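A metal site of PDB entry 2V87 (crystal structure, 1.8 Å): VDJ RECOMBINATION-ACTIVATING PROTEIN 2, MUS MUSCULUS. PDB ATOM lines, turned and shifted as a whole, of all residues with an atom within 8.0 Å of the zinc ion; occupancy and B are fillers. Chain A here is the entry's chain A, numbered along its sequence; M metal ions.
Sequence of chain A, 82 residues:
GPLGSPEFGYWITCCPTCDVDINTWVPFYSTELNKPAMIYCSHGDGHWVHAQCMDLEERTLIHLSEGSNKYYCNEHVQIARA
The zinc ion is bound by NE2 of His 47 (2.0 Å), ND1 of His 76 (2.1 Å), SG of Cys 41 (2.2 Å) and SG of Cys 73 (2.3 Å).
SG of Cys 73 sits close to N of Glu 75. SG of Cys 41 lies close to N of His 43 (3.5 Å).
The nearest printed residue that does not touch the zinc ion is His 43 (4.1 Å).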
ATOM      1  N   CYS A  14      10.817   0.879 -13.467  1.00  0.00           N
ATOM      2  CA  CYS A  14      11.132  -0.438 -12.937  1.00  0.00           C
ATOM      3  C   CYS A  14      10.787  -0.758 -11.492  1.00  0.00           C
ATOM      4  O   CYS A  14      10.669  -1.925 -11.126  1.00  0.00           O
ATOM      5  CB  CYS A  14      12.617  -0.772 -13.182  1.00  0.00           C
ATOM      6  SG  CYS A  14      13.769  -0.035 -12.015  1.00  0.00           S
ATOM      7  N   CYS A  15      10.653   0.268 -10.667  1.00  0.00           N
ATOM      8  CA  CYS A  15      10.326   0.063  -9.264  1.00  0.00           C
ATOM      9  C   CYS A  15       9.813   1.373  -8.668  1.00  0.00           C
ATOM     10  O   CYS A  15       9.908   2.412  -9.293  1.00  0.00           O
ATOM     11  CB  CYS A  15      11.563  -0.438  -8.493  1.00  0.00           C
ATOM     12  SG  CYS A  15      12.921   0.742  -8.372  1.00  0.00           S
ATOM     13  N   ILE A  39      18.683  -5.607 -15.748  1.00  0.00           N
ATOM     14  CA  ILE A  39      18.880  -6.969 -15.306  1.00  0.00           C
ATOM     15  C   ILE A  39      17.523  -7.599 -15.031  1.00  0.00           C
ATOM     16  O   ILE A  39      16.607  -6.954 -14.540  1.00  0.00           O
ATOM     17  CB  ILE A  39      19.792  -7.036 -14.055  1.00  0.00           C
ATOM     18  CG1 ILE A  39      20.030  -8.492 -13.645  1.00  0.00           C
ATOM     19  CG2 ILE A  39      19.182  -6.216 -12.921  1.00  0.00           C
ATOM     20  CD1 ILE A  39      21.176  -8.671 -12.670  1.00  0.00           C
ATOM     21  N   TYR A  40      17.411  -8.879 -15.362  1.00  0.00           N
ATOM     22  CA  TYR A  40      16.163  -9.609 -15.191  1.00  0.00           C
ATOM     23  C   TYR A  40      15.998 -10.162 -13.780  1.00  0.00           C
ATOM     24  O   TYR A  40      16.869 -10.856 -13.274  1.00  0.00           O
ATOM     25  CB  TYR A  40      16.103 -10.757 -16.208  1.00  0.00           C
ATOM     26  CG  TYR A  40      14.738 -11.383 -16.355  1.00  0.00           C
ATOM     27  CD1 TYR A  40      13.683 -10.681 -16.930  1.00  0.00           C
ATOM     28  CD2 TYR A  40      14.505 -12.692 -15.935  1.00  0.00           C
ATOM     29  CE1 TYR A  40      12.431 -11.276 -17.099  1.00  0.00           C
ATOM     30  CE2 TYR A  40      13.252 -13.294 -16.097  1.00  0.00           C
ATOM     31  CZ  TYR A  40      12.229 -12.574 -16.681  1.00  0.00           C
ATOM     32  OH  TYR A  40      10.991 -13.165 -16.860  1.00  0.00           O
ATOM     33  N   CYS A  41      14.869  -9.845 -13.153  1.00  0.00           N
ATOM     34  CA  CYS A  41      14.551 -10.342 -11.819  1.00  0.00           C
ATOM     35  C   CYS A  41      13.704 -11.603 -12.024  1.00  0.00           C
ATOM     36  O   CYS A  41      12.710 -11.566 -12.728  1.00  0.00           O
ATOM     37  CB  CYS A  41      13.747  -9.307 -11.039  1.00  0.00           C
ATOM     38  SG  CYS A  41      13.030  -9.949  -9.499  1.00  0.00           S
ATOM     39  N   SER A  42      14.105 -12.706 -11.411  1.00  0.00           N
ATOM     40  CA  SER A  42      13.394 -13.973 -11.575  1.00  0.00           C
ATOM     41  C   SER A  42      12.171 -14.192 -10.701  1.00  0.00           C
ATOM     42  O   SER A  42      11.585 -15.272 -10.738  1.00  0.00           O
ATOM     43  CB  SER A  42      14.369 -15.140 -11.373  1.00  0.00           C
ATOM     44  OG  SER A  42      15.354 -15.145 -12.399  1.00  0.00           O
ATOM     45  N   HIS A  43      11.776 -13.190  -9.923  1.00  0.00           N
ATOM     46  CA  HIS A  43      10.604 -13.331  -9.055  1.00  0.00           C
ATOM     47  C   HIS A  43       9.316 -13.555  -9.852  1.00  0.00           C
ATOM     48  O   HIS A  43       9.082 -12.898 -10.864  1.00  0.00           O
ATOM     49  CB  HIS A  43      10.411 -12.101  -8.178  1.00  0.00           C
ATOM     50  CG  HIS A  43       9.164 -12.139  -7.368  1.00  0.00           C
ATOM     51  ND1 HIS A  43       9.024 -12.945  -6.263  1.00  0.00           N
ATOM     52  CD2 HIS A  43       7.975 -11.508  -7.533  1.00  0.00           C
ATOM     53  CE1 HIS A  43       7.789 -12.818  -5.778  1.00  0.00           C
ATOM     54  NE2 HIS A  43       7.135 -11.951  -6.526  1.00  0.00           N
ATOM     55  N   GLY A  44       8.487 -14.468  -9.371  1.00  0.00           N
ATOM     56  CA  GLY A  44       7.228 -14.758 -10.036  1.00  0.00           C
ATOM     57  C   GLY A  44       7.414 -15.043 -11.508  1.00  0.00           C
ATOM     58  O   GLY A  44       8.202 -15.909 -11.868  1.00  0.00           O
ATOM     59  N   GLY A  46       8.716 -13.066 -13.499  1.00  0.00           N
ATOM     60  CA  GLY A  46       9.860 -12.297 -13.925  1.00  0.00           C
ATOM     61  C   GLY A  46       9.571 -10.912 -14.473  1.00  0.00           C
ATOM     62  O   GLY A  46       8.498 -10.639 -14.972  1.00  0.00           O
ATOM     63  N   HIS A  47      10.548 -10.021 -14.352  1.00  0.00           N
ATOM     64  CA  HIS A  47      10.395  -8.657 -14.845  1.00  0.00           C
ATOM     65  C   HIS A  47      11.761  -7.988 -14.932  1.00  0.00           C
ATOM     66  O   HIS A  47      12.701  -8.397 -14.263  1.00  0.00           O
ATOM     67  CB  HIS A  47       9.454  -7.853 -13.930  1.00  0.00           C
ATOM     68  CG  HIS A  47       9.998  -7.601 -12.558  1.00  0.00           C
ATOM     69  ND1 HIS A  47      10.275  -6.329 -12.090  1.00  0.00           N
ATOM     70  CD2 HIS A  47      10.301  -8.453 -11.548  1.00  0.00           C
ATOM     71  CE1 HIS A  47      10.727  -6.420 -10.853  1.00  0.00           C
ATOM     72  NE2 HIS A  47      10.747  -7.690 -10.495  1.00  0.00           N
ATOM     73  N   TRP A  48      11.865  -6.960 -15.760  1.00  0.00           N
ATOM     74  CA  TRP A  48      13.119  -6.244 -15.929  1.00  0.00           C
ATOM     75  C   TRP A  48      13.234  -5.000 -15.055  1.00  0.00           C
ATOM     76  O   TRP A  48      12.265  -4.286 -14.859  1.00  0.00           O
ATOM     77  CB  TRP A  48      13.282  -5.825 -17.399  1.00  0.00           C
ATOM     78  CG  TRP A  48      13.527  -6.969 -18.344  1.00  0.00           C
ATOM     79  CD1 TRP A  48      12.579  -7.678 -19.035  1.00  0.00           C
ATOM     80  CD2 TRP A  48      14.790  -7.511 -18.711  1.00  0.00           C
ATOM     81  NE1 TRP A  48      13.188  -8.619 -19.831  1.00  0.00           N
ATOM     82  CE2 TRP A  48      14.555  -8.540 -19.649  1.00  0.00           C
ATOM     83  CE3 TRP A  48      16.119  -7.222 -18.346  1.00  0.00           C
ATOM     84  CZ2 TRP A  48      15.582  -9.289 -20.220  1.00  0.00           C
ATOM     85  CZ3 TRP A  48      17.146  -7.971 -18.916  1.00  0.00           C
ATOM     86  CH2 TRP A  48      16.870  -8.992 -19.848  1.00  0.00           C
ATOM     87  N   VAL A  49      14.428  -4.742 -14.532  1.00  0.00           N
ATOM     88  CA  VAL A  49      14.676  -3.556 -13.720  1.00  0.00           C
ATOM     89  C   VAL A  49      15.983  -2.934 -14.169  1.00  0.00           C
ATOM     90  O   VAL A  49      16.820  -3.595 -14.761  1.00  0.00           O
ATOM     91  CB  VAL A  49      14.779  -3.886 -12.199  1.00  0.00           C
ATOM     92  CG1 VAL A  49      13.461  -4.437 -11.682  1.00  0.00           C
ATOM     93  CG2 VAL A  49      15.927  -4.855 -11.940  1.00  0.00           C
ATOM     94  N   MET A  54      18.801  -0.423  -8.696  1.00  0.00           N
ATOM     95  CA  MET A  54      18.994  -1.459  -7.685  1.00  0.00           C
ATOM     96  C   MET A  54      20.262  -1.196  -6.879  1.00  0.00           C
ATOM     97  O   MET A  54      20.608  -1.956  -6.001  1.00  0.00           O
ATOM     98  CB  MET A  54      19.124  -2.833  -8.357  1.00  0.00           C
ATOM     99  CG  MET A  54      17.915  -3.257  -9.175  1.00  0.00           C
ATOM    100  SD  MET A  54      16.450  -3.474  -8.171  1.00  0.00           S
ATOM    101  CE  MET A  54      15.490  -2.044  -8.633  1.00  0.00           C
ATOM    102  N   TYR A  71      18.854 -13.460 -10.593  1.00  0.00           N
ATOM    103  CA  TYR A  71      18.864 -12.234  -9.808  1.00  0.00           C
ATOM    104  C   TYR A  71      17.462 -11.890  -9.330  1.00  0.00           C
ATOM    105  O   TYR A  71      16.477 -12.129 -10.034  1.00  0.00           O
ATOM    106  CB  TYR A  71      19.419 -11.068 -10.652  1.00  0.00           C
ATOM    107  CG  TYR A  71      19.306  -9.724  -9.967  1.00  0.00           C
ATOM    108  CD1 TYR A  71      18.277  -8.840 -10.286  1.00  0.00           C
ATOM    109  CD2 TYR A  71      20.195  -9.365  -8.961  1.00  0.00           C
ATOM    110  CE1 TYR A  71      18.135  -7.630  -9.618  1.00  0.00           C
ATOM    111  CE2 TYR A  71      20.069  -8.147  -8.286  1.00  0.00           C
ATOM    112  CZ  TYR A  71      19.033  -7.290  -8.617  1.00  0.00           C
ATOM    113  OH  TYR A  71      18.895  -6.107  -7.933  1.00  0.00           O
ATOM    114  N   TYR A  72      17.383 -11.344  -8.118  1.00  0.00           N
ATOM    115  CA  TYR A  72      16.106 -10.928  -7.540  1.00  0.00           C
ATOM    116  C   TYR A  72      16.246  -9.475  -7.114  1.00  0.00           C
ATOM    117  O   TYR A  72      17.143  -9.140  -6.351  1.00  0.00           O
ATOM    118  CB  TYR A  72      15.748 -11.826  -6.352  1.00  0.00           C
ATOM    119  CG  TYR A  72      15.500 -13.249  -6.768  1.00  0.00           C
ATOM    120  CD1 TYR A  72      16.556 -14.159  -6.843  1.00  0.00           C
ATOM    121  CD2 TYR A  72      14.239 -13.682  -7.156  1.00  0.00           C
ATOM    122  CE1 TYR A  72      16.361 -15.455  -7.317  1.00  0.00           C
ATOM    123  CE2 TYR A  72      14.030 -14.975  -7.628  1.00  0.00           C
ATOM    124  CZ  TYR A  72      15.095 -15.852  -7.699  1.00  0.00           C
ATOM    125  OH  TYR A  72      14.903 -17.131  -8.170  1.00  0.00           O
ATOM    126  N   CYS A  73      15.356  -8.629  -7.615  1.00  0.00           N
ATOM    127  CA  CYS A  73      15.415  -7.203  -7.299  1.00  0.00           C
ATOM    128  C   CYS A  73      15.197  -6.936  -5.818  1.00  0.00           C
ATOM    129  O   CYS A  73      14.761  -7.813  -5.067  1.00  0.00           O
ATOM    130  CB  CYS A  73      14.406  -6.407  -8.127  1.00  0.00           C
ATOM    131  SG  CYS A  73      12.678  -6.587  -7.634  1.00  0.00           S
ATOM    132  N   ASN A  74      15.506  -5.718  -5.400  1.00  0.00           N
ATOM    133  CA  ASN A  74      15.393  -5.302  -4.009  1.00  0.00           C
ATOM    134  C   ASN A  74      13.990  -5.460  -3.428  1.00  0.00           C
ATOM    135  O   ASN A  74      13.841  -5.701  -2.244  1.00  0.00           O
ATOM    136  CB  ASN A  74      15.889  -3.851  -3.872  1.00  0.00           C
ATOM    137  CG  ASN A  74      17.364  -3.706  -4.256  1.00  0.00           C
ATOM    138  OD1 ASN A  74      17.859  -2.603  -4.462  1.00  0.00           O
ATOM    139  ND2 ASN A  74      18.060  -4.831  -4.342  1.00  0.00           N
ATOM    140  N   GLU A  75      12.964  -5.338  -4.273  1.00  0.00           N
ATOM    141  CA  GLU A  75      11.582  -5.478  -3.812  1.00  0.00           C
ATOM    142  C   GLU A  75      11.176  -6.929  -3.560  1.00  0.00           C
ATOM    143  O   GLU A  75      10.341  -7.198  -2.704  1.00  0.00           O
ATOM    144  CB  GLU A  75      10.614  -4.918  -4.861  1.00  0.00           C
ATOM    145  CG  GLU A  75      10.369  -3.427  -4.798  1.00  0.00           C
ATOM    146  CD  GLU A  75       9.415  -2.979  -5.883  1.00  0.00           C
ATOM    147  OE1 GLU A  75       9.839  -2.903  -7.060  1.00  0.00           O
ATOM    148  OE2 GLU A  75       8.229  -2.739  -5.566  1.00  0.00           O
ATOM    149  N   HIS A  76      11.768  -7.849  -4.308  1.00  0.00           N
ATOM    150  CA  HIS A  76      11.420  -9.271  -4.192  1.00  0.00           C
ATOM    151  C   HIS A  76      12.494 -10.170  -3.609  1.00  0.00           C
ATOM    152  O   HIS A  76      12.259 -11.348  -3.368  1.00  0.00           O
ATOM    153  CB  HIS A  76      11.043  -9.804  -5.575  1.00  0.00           C
ATOM    154  CG  HIS A  76       9.930  -9.058  -6.248  1.00  0.00           C
ATOM    155  ND1 HIS A  76       9.977  -8.681  -7.568  1.00  0.00           N
ATOM    156  CD2 HIS A  76       8.719  -8.659  -5.781  1.00  0.00           C
ATOM    157  CE1 HIS A  76       8.842  -8.094  -7.897  1.00  0.00           C
ATOM    158  NE2 HIS A  76       8.064  -8.069  -6.831  1.00  0.00           N
ATOM    159  N   VAL A  77      13.686  -9.622  -3.390  1.00  0.00           N
ATOM    160  CA  VAL A  77      14.798 -10.424  -2.880  1.00  0.00           C
ATOM    161  C   VAL A  77      14.569 -11.148  -1.564  1.00  0.00           C
ATOM    162  O   VAL A  77      15.176 -12.184  -1.308  1.00  0.00           O
ATOM    163  CB  VAL A  77      16.086  -9.573  -2.770  1.00  0.00           C
ATOM    164  CG1 VAL A  77      16.017  -8.688  -1.526  1.00  0.00           C
ATOM    165  CG2 VAL A  77      17.300 -10.481  -2.727  1.00  0.00           C
ATOM    166  N   ILE A  79      11.617 -12.356  -0.534  1.00  0.00           N
ATOM    167  CA  ILE A  79      10.474 -13.254  -0.586  1.00  0.00           C
ATOM    168  C   ILE A  79      10.818 -14.727  -0.600  1.00  0.00           C
ATOM    169  O   ILE A  79      11.654 -15.183  -1.384  1.00  0.00           O
ATOM    170  CB  ILE A  79       9.583 -12.948  -1.789  1.00  0.00           C
ATOM    171  CG1 ILE A  79       8.990 -11.543  -1.642  1.00  0.00           C
ATOM    172  CG2 ILE A  79       8.461 -13.987  -1.891  1.00  0.00           C
ATOM    173  CD1 ILE A  79       8.140 -11.103  -2.800  1.00  0.00           C
HETATM  174 ZN    ZN M   1      11.679  -8.299  -8.820  1.00  0.00          ZN
